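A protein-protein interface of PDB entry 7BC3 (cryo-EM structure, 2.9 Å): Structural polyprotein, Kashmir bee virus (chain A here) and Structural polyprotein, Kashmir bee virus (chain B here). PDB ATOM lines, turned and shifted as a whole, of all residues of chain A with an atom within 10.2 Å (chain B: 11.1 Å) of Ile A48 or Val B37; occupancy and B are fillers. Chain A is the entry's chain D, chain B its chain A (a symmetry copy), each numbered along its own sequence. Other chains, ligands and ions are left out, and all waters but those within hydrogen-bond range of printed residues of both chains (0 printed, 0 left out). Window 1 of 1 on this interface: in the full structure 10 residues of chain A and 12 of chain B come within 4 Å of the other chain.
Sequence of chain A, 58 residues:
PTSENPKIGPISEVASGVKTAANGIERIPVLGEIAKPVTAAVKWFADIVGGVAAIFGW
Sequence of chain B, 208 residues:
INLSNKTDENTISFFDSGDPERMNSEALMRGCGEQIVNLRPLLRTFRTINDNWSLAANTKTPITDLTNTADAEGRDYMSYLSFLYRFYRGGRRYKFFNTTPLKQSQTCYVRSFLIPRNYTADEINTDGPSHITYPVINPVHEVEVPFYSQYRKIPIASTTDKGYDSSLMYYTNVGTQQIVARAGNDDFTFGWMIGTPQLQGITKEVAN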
ATOM      1  N   VAL A  38     -14.595  19.073  39.596  1.00  0.00           N
ATOM      2  CA  VAL A  38     -14.813  20.007  38.501  1.00  0.00           C
ATOM      3  C   VAL A  38     -13.617  19.896  37.569  1.00  0.00           C
ATOM      4  O   VAL A  38     -12.661  20.673  37.664  1.00  0.00           O
ATOM      5  CB  VAL A  38     -14.999  21.447  39.012  1.00  0.00           C
ATOM      6  CG1 VAL A  38     -15.408  22.369  37.875  1.00  0.00           C
ATOM      7  CG2 VAL A  38     -16.025  21.491  40.134  1.00  0.00           C
ATOM      8  N   THR A  39     -13.675  18.930  36.657  1.00  0.00           N
ATOM      9  CA  THR A  39     -12.568  18.617  35.766  1.00  0.00           C
ATOM     10  C   THR A  39     -13.144  18.038  34.480  1.00  0.00           C
ATOM     11  O   THR A  39     -14.364  17.952  34.309  1.00  0.00           O
ATOM     12  CB  THR A  39     -11.594  17.630  36.421  1.00  0.00           C
ATOM     13  OG1 THR A  39     -12.327  16.529  36.968  1.00  0.00           O
ATOM     14  CG2 THR A  39     -10.792  18.293  37.521  1.00  0.00           C
ATOM     15  N   ALA A  40     -12.257  17.618  33.579  1.00  0.00           N
ATOM     16  CA  ALA A  40     -12.675  16.873  32.401  1.00  0.00           C
ATOM     17  C   ALA A  40     -13.125  15.457  32.732  1.00  0.00           C
ATOM     18  O   ALA A  40     -13.476  14.709  31.813  1.00  0.00           O
ATOM     19  CB  ALA A  40     -11.538  16.831  31.383  1.00  0.00           C
ATOM     20  N   ALA A  41     -13.122  15.071  34.011  1.00  0.00           N
ATOM     21  CA  ALA A  41     -13.650  13.772  34.404  1.00  0.00           C
ATOM     22  C   ALA A  41     -15.150  13.674  34.183  1.00  0.00           C
ATOM     23  O   ALA A  41     -15.671  12.566  34.022  1.00  0.00           O
ATOM     24  CB  ALA A  41     -13.333  13.499  35.873  1.00  0.00           C
ATOM     25  N   VAL A  42     -15.848  14.796  34.181  1.00  0.00           N
ATOM     26  CA  VAL A  42     -17.280  14.831  33.925  1.00  0.00           C
ATOM     27  C   VAL A  42     -17.494  15.063  32.437  1.00  0.00           C
ATOM     28  O   VAL A  42     -16.779  15.849  31.805  1.00  0.00           O
ATOM     29  CB  VAL A  42     -17.960  15.919  34.775  1.00  0.00           C
ATOM     30  CG1 VAL A  42     -19.462  15.819  34.664  1.00  0.00           C
ATOM     31  CG2 VAL A  42     -17.529  15.786  36.223  1.00  0.00           C
ATOM     32  N   LYS A  43     -18.487  14.376  31.876  1.00  0.00           N
ATOM     33  CA  LYS A  43     -18.638  14.348  30.426  1.00  0.00           C
ATOM     34  C   LYS A  43     -18.997  15.723  29.878  1.00  0.00           C
ATOM     35  O   LYS A  43     -18.335  16.227  28.964  1.00  0.00           O
ATOM     36  CB  LYS A  43     -19.695  13.317  30.038  1.00  0.00           C
ATOM     37  CG  LYS A  43     -19.974  13.237  28.550  1.00  0.00           C
ATOM     38  CD  LYS A  43     -18.765  12.762  27.782  1.00  0.00           C
ATOM     39  CE  LYS A  43     -19.096  12.557  26.320  1.00  0.00           C
ATOM     40  NZ  LYS A  43     -19.015  13.825  25.554  1.00  0.00           N
ATOM     41  N   TRP A  44     -20.048  16.344  30.414  1.00  0.00           N
ATOM     42  CA  TRP A  44     -20.483  17.628  29.875  1.00  0.00           C
ATOM     43  C   TRP A  44     -19.460  18.723  30.153  1.00  0.00           C
ATOM     44  O   TRP A  44     -19.256  19.615  29.321  1.00  0.00           O
ATOM     45  CB  TRP A  44     -21.853  18.004  30.440  1.00  0.00           C
ATOM     46  CG  TRP A  44     -21.946  17.982  31.930  1.00  0.00           C
ATOM     47  CD1 TRP A  44     -22.268  16.916  32.712  1.00  0.00           C
ATOM     48  CD2 TRP A  44     -21.734  19.083  32.817  1.00  0.00           C
ATOM     49  NE1 TRP A  44     -22.261  17.282  34.034  1.00  0.00           N
ATOM     50  CE2 TRP A  44     -21.937  18.608  34.125  1.00  0.00           C
ATOM     51  CE3 TRP A  44     -21.388  20.424  32.633  1.00  0.00           C
ATOM     52  CZ2 TRP A  44     -21.807  19.425  35.241  1.00  0.00           C
ATOM     53  CZ3 TRP A  44     -21.258  21.231  33.742  1.00  0.00           C
ATOM     54  CH2 TRP A  44     -21.467  20.730  35.029  1.00  0.00           C
ATOM     55  N   PHE A  45     -18.789  18.667  31.302  1.00  0.00           N
ATOM     56  CA  PHE A  45     -17.777  19.674  31.599  1.00  0.00           C
ATOM     57  C   PHE A  45     -16.578  19.536  30.670  1.00  0.00           C
ATOM     58  O   PHE A  45     -16.007  20.541  30.226  1.00  0.00           O
ATOM     59  CB  PHE A  45     -17.340  19.565  33.055  1.00  0.00           C
ATOM     60  CG  PHE A  45     -16.540  20.736  33.530  1.00  0.00           C
ATOM     61  CD1 PHE A  45     -17.166  21.896  33.941  1.00  0.00           C
ATOM     62  CD2 PHE A  45     -15.159  20.681  33.555  1.00  0.00           C
ATOM     63  CE1 PHE A  45     -16.432  22.975  34.373  1.00  0.00           C
ATOM     64  CE2 PHE A  45     -14.421  21.758  33.987  1.00  0.00           C
ATOM     65  CZ  PHE A  45     -15.057  22.906  34.396  1.00  0.00           C
ATOM     66  N   ALA A  46     -16.173  18.299  30.382  1.00  0.00           N
ATOM     67  CA  ALA A  46     -15.131  18.077  29.389  1.00  0.00           C
ATOM     68  C   ALA A  46     -15.576  18.570  28.021  1.00  0.00           C
ATOM     69  O   ALA A  46     -14.791  19.176  27.284  1.00  0.00           O
ATOM     70  CB  ALA A  46     -14.771  16.594  29.334  1.00  0.00           C
ATOM     71  N   ASP A  47     -16.835  18.319  27.667  1.00  0.00           N
ATOM     72  CA  ASP A  47     -17.376  18.826  26.413  1.00  0.00           C
ATOM     73  C   ASP A  47     -17.241  20.339  26.332  1.00  0.00           C
ATOM     74  O   ASP A  47     -16.867  20.884  25.289  1.00  0.00           O
ATOM     75  CB  ASP A  47     -18.841  18.417  26.290  1.00  0.00           C
ATOM     76  CG  ASP A  47     -19.015  16.985  25.833  1.00  0.00           C
ATOM     77  OD1 ASP A  47     -18.190  16.132  26.213  1.00  0.00           O
ATOM     78  OD2 ASP A  47     -19.997  16.714  25.112  1.00  0.00           O
ATOM     79  N   ILE A  48     -17.543  21.032  27.428  1.00  0.00           N
ATOM     80  CA  ILE A  48     -17.485  22.490  27.426  1.00  0.00           C
ATOM     81  C   ILE A  48     -16.043  22.965  27.308  1.00  0.00           C
ATOM     82  O   ILE A  48     -15.675  23.664  26.358  1.00  0.00           O
ATOM     83  CB  ILE A  48     -18.148  23.064  28.689  1.00  0.00           C
ATOM     84  CG1 ILE A  48     -19.602  22.599  28.802  1.00  0.00           C
ATOM     85  CG2 ILE A  48     -18.075  24.581  28.669  1.00  0.00           C
ATOM     86  CD1 ILE A  48     -20.570  23.392  27.980  1.00  0.00           C
ATOM     87  N   VAL A  49     -15.205  22.593  28.279  1.00  0.00           N
ATOM     88  CA  VAL A  49     -13.852  23.134  28.341  1.00  0.00           C
ATOM     89  C   VAL A  49     -12.963  22.647  27.211  1.00  0.00           C
ATOM     90  O   VAL A  49     -11.938  23.276  26.929  1.00  0.00           O
ATOM     91  CB  VAL A  49     -13.197  22.802  29.694  1.00  0.00           C
ATOM     92  CG1 VAL A  49     -14.062  23.313  30.831  1.00  0.00           C
ATOM     93  CG2 VAL A  49     -12.959  21.311  29.819  1.00  0.00           C
ATOM     94  N   GLY A  50     -13.323  21.549  26.555  1.00  0.00           N
ATOM     95  CA  GLY A  50     -12.644  21.118  25.357  1.00  0.00           C
ATOM     96  C   GLY A  50     -13.209  21.714  24.096  1.00  0.00           C
ATOM     97  O   GLY A  50     -12.696  21.448  23.005  1.00  0.00           O
ATOM     98  N   GLY A  51     -14.255  22.526  24.218  1.00  0.00           N
ATOM     99  CA  GLY A  51     -14.888  23.118  23.055  1.00  0.00           C
ATOM    100  C   GLY A  51     -15.209  22.113  21.973  1.00  0.00           C
ATOM    101  O   GLY A  51     -14.610  22.159  20.893  1.00  0.00           O
ATOM    102  N   VAL A  52     -16.118  21.176  22.250  1.00  0.00           N
ATOM    103  CA  VAL A  52     -16.579  20.298  21.189  1.00  0.00           C
ATOM    104  C   VAL A  52     -17.662  21.012  20.386  1.00  0.00           C
ATOM    105  O   VAL A  52     -18.256  22.004  20.826  1.00  0.00           O
ATOM    106  CB  VAL A  52     -17.090  18.956  21.737  1.00  0.00           C
ATOM    107  CG1 VAL A  52     -15.969  18.217  22.440  1.00  0.00           C
ATOM    108  CG2 VAL A  52     -18.268  19.161  22.668  1.00  0.00           C
ATOM    109  N   ALA A  53     -17.915  20.499  19.185  1.00  0.00           N
ATOM    110  CA  ALA A  53     -18.842  21.143  18.268  1.00  0.00           C
ATOM    111  C   ALA A  53     -20.301  20.868  18.599  1.00  0.00           C
ATOM    112  O   ALA A  53     -21.181  21.454  17.960  1.00  0.00           O
ATOM    113  CB  ALA A  53     -18.550  20.690  16.838  1.00  0.00           C
ATOM    114  N   ALA A  54     -20.581  20.006  19.575  1.00  0.00           N
ATOM    115  CA  ALA A  54     -21.962  19.666  19.888  1.00  0.00           C
ATOM    116  C   ALA A  54     -22.603  20.683  20.821  1.00  0.00           C
ATOM    117  O   ALA A  54     -23.806  20.941  20.714  1.00  0.00           O
ATOM    118  CB  ALA A  54     -22.031  18.273  20.507  1.00  0.00           C
ATOM    119  N   ILE A  55     -21.826  21.267  21.735  1.00  0.00           N
ATOM    120  CA  ILE A  55     -22.354  22.298  22.619  1.00  0.00           C
ATOM    121  C   ILE A  55     -22.788  23.540  21.862  1.00  0.00           C
ATOM    122  O   ILE A  55     -23.471  24.398  22.431  1.00  0.00           O
ATOM    123  CB  ILE A  55     -21.310  22.677  23.689  1.00  0.00           C
ATOM    124  CG1 ILE A  55     -20.004  23.125  23.037  1.00  0.00           C
ATOM    125  CG2 ILE A  55     -21.041  21.502  24.604  1.00  0.00           C
ATOM    126  CD1 ILE A  55     -19.209  24.079  23.884  1.00  0.00           C
ATOM    127  N   PHE A  56     -22.406  23.656  20.592  1.00  0.00           N
ATOM    128  CA  PHE A  56     -22.830  24.748  19.732  1.00  0.00           C
ATOM    129  C   PHE A  56     -23.981  24.359  18.818  1.00  0.00           C
ATOM    130  O   PHE A  56     -24.520  25.224  18.124  1.00  0.00           O
ATOM    131  CB  PHE A  56     -21.653  25.235  18.886  1.00  0.00           C
ATOM    132  CG  PHE A  56     -20.468  25.676  19.690  1.00  0.00           C
ATOM    133  CD1 PHE A  56     -20.558  26.762  20.538  1.00  0.00           C
ATOM    134  CD2 PHE A  56     -19.262  25.009  19.593  1.00  0.00           C
ATOM    135  CE1 PHE A  56     -19.472  27.171  21.276  1.00  0.00           C
ATOM    136  CE2 PHE A  56     -18.172  25.414  20.329  1.00  0.00           C
ATOM    137  CZ  PHE A  56     -18.277  26.497  21.171  1.00  0.00           C
ATOM    138  N   GLY A  57     -24.362  23.088  18.796  1.00  0.00           N
ATOM    139  CA  GLY A  57     -25.437  22.623  17.953  1.00  0.00           C
ATOM    140  C   GLY A  57     -25.007  21.985  16.654  1.00  0.00           C
ATOM    141  O   GLY A  57     -25.860  21.747  15.793  1.00  0.00           O
ATOM    142  N   GLU B  21     -16.745  32.023  37.166  1.00  0.00           N
ATOM    143  CA  GLU B  21     -16.833  30.724  36.512  1.00  0.00           C
ATOM    144  C   GLU B  21     -16.650  29.594  37.516  1.00  0.00           C
ATOM    145  O   GLU B  21     -17.312  28.557  37.419  1.00  0.00           O
ATOM    146  CB  GLU B  21     -15.800  30.626  35.394  1.00  0.00           C
ATOM    147  CG  GLU B  21     -15.978  31.672  34.305  1.00  0.00           C
ATOM    148  CD  GLU B  21     -17.298  31.533  33.572  1.00  0.00           C
ATOM    149  OE1 GLU B  21     -17.775  30.390  33.413  1.00  0.00           O
ATOM    150  OE2 GLU B  21     -17.858  32.568  33.152  1.00  0.00           O
ATOM    151  N   ASN B  24     -19.970  29.364  39.336  1.00  0.00           N
ATOM    152  CA  ASN B  24     -20.986  28.869  38.419  1.00  0.00           C
ATOM    153  C   ASN B  24     -20.826  27.377  38.170  1.00  0.00           C
ATOM    154  O   ASN B  24     -21.809  26.630  38.171  1.00  0.00           O
ATOM    155  CB  ASN B  24     -20.905  29.642  37.107  1.00  0.00           C
ATOM    156  CG  ASN B  24     -21.508  31.025  37.211  1.00  0.00           C
ATOM    157  OD1 ASN B  24     -21.975  31.436  38.271  1.00  0.00           O
ATOM    158  ND2 ASN B  24     -21.491  31.758  36.109  1.00  0.00           N
ATOM    159  N   SER B  25     -19.592  26.924  37.954  1.00  0.00           N
ATOM    160  CA  SER B  25     -19.352  25.513  37.687  1.00  0.00           C
ATOM    161  C   SER B  25     -19.660  24.665  38.912  1.00  0.00           C
ATOM    162  O   SER B  25     -20.216  23.568  38.791  1.00  0.00           O
ATOM    163  CB  SER B  25     -17.907  25.322  37.235  1.00  0.00           C
ATOM    164  OG  SER B  25     -17.710  25.859  35.939  1.00  0.00           O
ATOM    165  N   LEU B  28     -23.402  24.393  39.101  1.00  0.00           N
ATOM    166  CA  LEU B  28     -23.901  23.436  38.119  1.00  0.00           C
ATOM    167  C   LEU B  28     -23.644  22.006  38.568  1.00  0.00           C
ATOM    168  O   LEU B  28     -24.519  21.143  38.447  1.00  0.00           O
ATOM    169  CB  LEU B  28     -23.247  23.684  36.764  1.00  0.00           C
ATOM    170  CG  LEU B  28     -23.525  25.036  36.117  1.00  0.00           C
ATOM    171  CD1 LEU B  28     -22.555  25.263  34.981  1.00  0.00           C
ATOM    172  CD2 LEU B  28     -24.953  25.117  35.635  1.00  0.00           C
ATOM    173  N   MET B  29     -22.444  21.737  39.085  1.00  0.00           N
ATOM    174  CA  MET B  29     -22.137  20.401  39.575  1.00  0.00           C
ATOM    175  C   MET B  29     -23.073  19.990  40.698  1.00  0.00           C
ATOM    176  O   MET B  29     -23.352  18.799  40.870  1.00  0.00           O
ATOM    177  CB  MET B  29     -20.691  20.345  40.062  1.00  0.00           C
ATOM    178  CG  MET B  29     -19.658  20.309  38.958  1.00  0.00           C
ATOM    179  SD  MET B  29     -19.774  18.846  37.918  1.00  0.00           S
ATOM    180  CE  MET B  29     -18.479  19.204  36.740  1.00  0.00           C
ATOM    181  N   CYS B  32     -27.554  21.436  38.827  1.00  0.00           N
ATOM    182  CA  CYS B  32     -28.090  21.282  37.478  1.00  0.00           C
ATOM    183  C   CYS B  32     -27.665  19.984  36.815  1.00  0.00           C
ATOM    184  O   CYS B  32     -28.517  19.251  36.298  1.00  0.00           O
ATOM    185  CB  CYS B  32     -27.676  22.469  36.599  1.00  0.00           C
ATOM    186  SG  CYS B  32     -28.431  22.449  34.961  1.00  0.00           S
ATOM    187  N   GLY B  33     -26.373  19.671  36.816  1.00  0.00           N
ATOM    188  CA  GLY B  33     -25.868  18.509  36.119  1.00  0.00           C
ATOM    189  C   GLY B  33     -25.539  18.728  34.659  1.00  0.00           C
ATOM    190  O   GLY B  33     -25.045  17.799  34.009  1.00  0.00           O
ATOM    191  N   GLU B  34     -25.792  19.917  34.122  1.00  0.00           N
ATOM    192  CA  GLU B  34     -25.492  20.218  32.730  1.00  0.00           C
ATOM    193  C   GLU B  34     -25.238  21.713  32.614  1.00  0.00           C
ATOM    194  O   GLU B  34     -25.377  22.462  33.584  1.00  0.00           O
ATOM    195  CB  GLU B  34     -26.626  19.774  31.800  1.00  0.00           C
ATOM    196  CG  GLU B  34     -27.982  20.345  32.158  1.00  0.00           C
ATOM    197  CD  GLU B  34     -29.131  19.466  31.719  1.00  0.00           C
ATOM    198  OE1 GLU B  34     -28.891  18.299  31.345  1.00  0.00           O
ATOM    199  OE2 GLU B  34     -30.281  19.946  31.744  1.00  0.00           O
ATOM    200  N   GLN B  35     -24.859  22.140  31.411  1.00  0.00           N
ATOM    201  CA  GLN B  35     -24.556  23.541  31.149  1.00  0.00           C
ATOM    202  C   GLN B  35     -25.003  23.894  29.741  1.00  0.00           C
ATOM    203  O   GLN B  35     -24.522  23.304  28.770  1.00  0.00           O
ATOM    204  CB  GLN B  35     -23.063  23.829  31.320  1.00  0.00           C
ATOM    205  CG  GLN B  35     -22.746  25.297  31.513  1.00  0.00           C
ATOM    206  CD  GLN B  35     -21.267  25.560  31.678  1.00  0.00           C
ATOM    207  OE1 GLN B  35     -20.512  24.691  32.111  1.00  0.00           O
ATOM    208  NE2 GLN B  35     -20.845  26.766  31.332  1.00  0.00           N
ATOM    209  N   ILE B  36     -25.915  24.853  29.636  1.00  0.00           N
ATOM    210  CA  ILE B  36     -26.389  25.364  28.357  1.00  0.00           C
ATOM    211  C   ILE B  36     -25.624  26.642  28.054  1.00  0.00           C
ATOM    212  O   ILE B  36     -25.726  27.627  28.796  1.00  0.00           O
ATOM    213  CB  ILE B  36     -27.904  25.616  28.374  1.00  0.00           C
ATOM    214  CG1 ILE B  36     -28.650  24.375  28.862  1.00  0.00           C
ATOM    215  CG2 ILE B  36     -28.390  26.004  26.992  1.00  0.00           C
ATOM    216  CD1 ILE B  36     -30.049  24.647  29.328  1.00  0.00           C
ATOM    217  N   VAL B  37     -24.854  26.627  26.968  1.00  0.00           N
ATOM    218  CA  VAL B  37     -24.043  27.772  26.573  1.00  0.00           C
ATOM    219  C   VAL B  37     -24.424  28.317  25.208  1.00  0.00           C
ATOM    220  O   VAL B  37     -23.892  29.364  24.808  1.00  0.00           O
ATOM    221  CB  VAL B  37     -22.539  27.425  26.597  1.00  0.00           C
ATOM    222  CG1 VAL B  37     -22.143  26.903  27.960  1.00  0.00           C
ATOM    223  CG2 VAL B  37     -22.211  26.405  25.526  1.00  0.00           C
ATOM    224  N   ASN B  38     -25.320  27.655  24.484  1.00  0.00           N
ATOM    225  CA  ASN B  38     -25.748  28.106  23.171  1.00  0.00           C
ATOM    226  C   ASN B  38     -27.204  27.714  22.985  1.00  0.00           C
ATOM    227  O   ASN B  38     -27.712  26.811  23.653  1.00  0.00           O
ATOM    228  CB  ASN B  38     -24.868  27.512  22.066  1.00  0.00           C
ATOM    229  CG  ASN B  38     -25.164  28.095  20.704  1.00  0.00           C
ATOM    230  OD1 ASN B  38     -26.307  28.101  20.250  1.00  0.00           O
ATOM    231  ND2 ASN B  38     -24.128  28.587  20.041  1.00  0.00           N
ATOM    232  N   LEU B  39     -27.873  28.407  22.068  1.00  0.00           N
ATOM    233  CA  LEU B  39     -29.304  28.240  21.862  1.00  0.00           C
ATOM    234  C   LEU B  39     -29.641  27.410  20.630  1.00  0.00           C
ATOM    235  O   LEU B  39     -30.824  27.176  20.365  1.00  0.00           O
ATOM    236  CB  LEU B  39     -29.973  29.612  21.767  1.00  0.00           C
ATOM    237  CG  LEU B  39     -29.797  30.464  23.026  1.00  0.00           C
ATOM    238  CD1 LEU B  39     -29.967  31.938  22.722  1.00  0.00           C
ATOM    239  CD2 LEU B  39     -30.769  30.025  24.102  1.00  0.00           C
ATOM    240  N   ARG B  40     -28.643  26.962  19.877  1.00  0.00           N
ATOM    241  CA  ARG B  40     -28.861  26.024  18.783  1.00  0.00           C
ATOM    242  C   ARG B  40     -29.237  24.649  19.326  1.00  0.00           C
ATOM    243  O   ARG B  40     -30.126  23.987  18.773  1.00  0.00           O
ATOM    244  CB  ARG B  40     -27.614  25.920  17.909  1.00  0.00           C
ATOM    245  CG  ARG B  40     -27.576  26.931  16.797  1.00  0.00           C
ATOM    246  CD  ARG B  40     -26.398  26.717  15.880  1.00  0.00           C
ATOM    247  NE  ARG B  40     -25.991  27.974  15.262  1.00  0.00           N
ATOM    248  CZ  ARG B  40     -25.039  28.773  15.734  1.00  0.00           C
ATOM    249  NH1 ARG B  40     -24.371  28.453  16.830  1.00  0.00           N
ATOM    250  NH2 ARG B  40     -24.756  29.899  15.099  1.00  0.00           N
ATOM    251  N   PRO B  41     -28.573  24.175  20.381  1.00  0.00           N
ATOM    252  CA  PRO B  41     -29.019  22.925  21.011  1.00  0.00           C
ATOM    253  C   PRO B  41     -30.505  22.893  21.292  1.00  0.00           C
ATOM    254  O   PRO B  41     -31.118  21.820  21.239  1.00  0.00           O
ATOM    255  CB  PRO B  41     -28.194  22.891  22.300  1.00  0.00           C
ATOM    256  CG  PRO B  41     -26.938  23.559  21.930  1.00  0.00           C
ATOM    257  CD  PRO B  41     -27.326  24.667  20.992  1.00  0.00           C
ATOM    258  N   LEU B  42     -31.109  24.044  21.580  1.00  0.00           N
ATOM    259  CA  LEU B  42     -32.549  24.103  21.785  1.00  0.00           C
ATOM    260  C   LEU B  42     -33.310  23.902  20.484  1.00  0.00           C
ATOM    261  O   LEU B  42     -34.446  23.412  20.502  1.00  0.00           O
ATOM    262  CB  LEU B  42     -32.928  25.440  22.415  1.00  0.00           C
ATOM    263  CG  LEU B  42     -32.310  25.723  23.782  1.00  0.00           C
ATOM    264  CD1 LEU B  42     -32.888  26.995  24.363  1.00  0.00           C
ATOM    265  CD2 LEU B  42     -32.519  24.557  24.728  1.00  0.00           C
ATOM    266  N   LEU B  43     -32.710  24.273  19.355  1.00  0.00           N
ATOM    267  CA  LEU B  43     -33.279  23.946  18.057  1.00  0.00           C
ATOM    268  C   LEU B  43     -33.060  22.487  17.696  1.00  0.00           C
ATOM    269  O   LEU B  43     -33.779  21.953  16.847  1.00  0.00           O
ATOM    270  CB  LEU B  43     -32.669  24.838  16.981  1.00  0.00           C
ATOM    271  CG  LEU B  43     -32.681  26.324  17.319  1.00  0.00           C
ATOM    272  CD1 LEU B  43     -32.016  27.121  16.224  1.00  0.00           C
ATOM    273  CD2 LEU B  43     -34.100  26.793  17.548  1.00  0.00           C
ATOM    274  N   LEU B  81     -37.399  31.955  19.500  1.00  0.00           N
ATOM    275  CA  LEU B  81     -36.106  32.496  19.109  1.00  0.00           C
ATOM    276  C   LEU B  81     -36.162  33.213  17.768  1.00  0.00           C
ATOM    277  O   LEU B  81     -35.392  34.150  17.541  1.00  0.00           O
ATOM    278  CB  LEU B  81     -35.070  31.376  19.059  1.00  0.00           C
ATOM    279  CG  LEU B  81     -34.821  30.662  20.388  1.00  0.00           C
ATOM    280  CD1 LEU B  81     -33.868  29.500  20.203  1.00  0.00           C
ATOM    281  CD2 LEU B  81     -34.285  31.630  21.424  1.00  0.00           C
ATOM    282  N   TYR B  85     -34.405  37.141  15.517  1.00  0.00           N
ATOM    283  CA  TYR B  85     -33.578  37.102  14.326  1.00  0.00           C
ATOM    284  C   TYR B  85     -34.428  37.423  13.109  1.00  0.00           C
ATOM    285  O   TYR B  85     -35.652  37.555  13.186  1.00  0.00           O
ATOM    286  CB  TYR B  85     -32.903  35.737  14.164  1.00  0.00           C
ATOM    287  CG  TYR B  85     -32.087  35.302  15.362  1.00  0.00           C
ATOM    288  CD1 TYR B  85     -30.730  35.564  15.434  1.00  0.00           C
ATOM    289  CD2 TYR B  85     -32.673  34.617  16.412  1.00  0.00           C
ATOM    290  CE1 TYR B  85     -29.985  35.173  16.514  1.00  0.00           C
ATOM    291  CE2 TYR B  85     -31.931  34.219  17.500  1.00  0.00           C
ATOM    292  CZ  TYR B  85     -30.588  34.503  17.546  1.00  0.00           C
ATOM    293  OH  TYR B  85     -29.837  34.109  18.625  1.00  0.00           O
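Thr A39 touches none of the printed residues of chain B.
Ala A40 touches none of the printed residues of chain B.
Of the printed residues of chain B, Val A42 touches Met B29 (3.6 Å).
Of chain B, only Ser B25 and Met B29 come within 4 Å of Phe A45.
No residue of chain B comes within 4 Å of Ala A46.
Of the printed residues of chain B, Ile A48 touches Val B37 (3.8 Å).
No residue of chain B comes within 4 Å of Val A49.
No residue of chain B comes within 4 Å of Gly A51.
No residue of chain B comes within 4 Å of Val A52.
Of chain B, only Val B37, Asn B38 and Pro B41 come within 4 Å of Ile A55.
Of the printed residues of chain A, Leu B28 touches Trp A44 (3.9 Å).
Of the printed residues of chain A, Gly B33 touches Trp A44.
Val B37 touches just these residues of chain A: Ile A48 (3.8 Å) and Ile A55 (3.9 Å).
Of chain A, only Ile A55 and Phe A56 come within 4 Å of Asn B38.
The nearest printed residue of chain B that does not touch Gly A57 is Pro B41 (4.01 Å).
O of Glu B21 is in hydrogen-bond range of OG of Ser B25, at 3.1 Å.
The backbone carbonyl oxygen of Leu B28 sits at hydrogen-bond distance from the backbone NH of Gly B33 (2.9 Å).
The side-chain sulfur of Cys B32 lies within hydrogen-bond range of the backbone carbonyl oxygen of Glu B34 (3.4 Å).
The side-chain amide oxygen (OD1) of Asn B38 lies within hydrogen-bond range of the backbone NH (N) of Arg B40 (2.6 Å).
Of the 20 printed residues of chain A, 8 touch a printed residue of chain B.
Printed residues of chain A that touch a printed residue of chain B: Val A38, Val A42, Trp A44, Phe A45, Ile A48, Ile A55, Phe A56 and Gly A57.
Hydrophobic or aromatic side chains of chain A that line the printed part of chain B: Val A38, Val A42, Trp A44, Phe A45 and Ile A48.
Printed residues of chain B that touch a printed residue of chain A: Ser B25, Leu B28, Met B29, Gly B33, Glu B34, Gln B35, Val B37, Asn B38, Arg B40 and Pro B41.
Along chain B the printed residues that touch a printed residue of chain A span positions 25 to 41.
Among the printed residues, no Asp or Glu carboxylate lies within 4 Å of a Lys or Arg side-chain nitrogen of the other chain.
Among the printed residues, merely in contact across the chains: Trp A44 with Met B29 (3.4 Å), Ile A55 with Asn B38 (3.4 Å), Phe A45 with Ser B25 (3.5 Å), Val A42 with Met B29 (3.6 Å), Ile A55 with Pro B41 (3.6 Å), Ile A48 with Val B37 (3.8 Å), Trp A44 with Leu B28 (3.9 Å), Phe A45 with Met B29 (3.9 Å), Phe A56 with Asn B38 (3.9 Å), Trp A44 with Gln B35 (3.9 Å), Ile A55 with Val B37 (3.9 Å), Val A38 with Ser B25 (3.9 Å), Trp A44 with Glu B34 (3.9 Å), Gly A57 with Arg B40 (3.95 Å) and Val A38 with Met B29 (3.997 Å).
The indole nitrogen (NE1) of Trp A44 is in hydrogen-bond range of the backbone carbonyl oxygen (O) of Gly B33.
The guanidinium group of Arg B40 sits close to the backbone carbonyl oxygen of Phe A56, at 3.5 Å.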
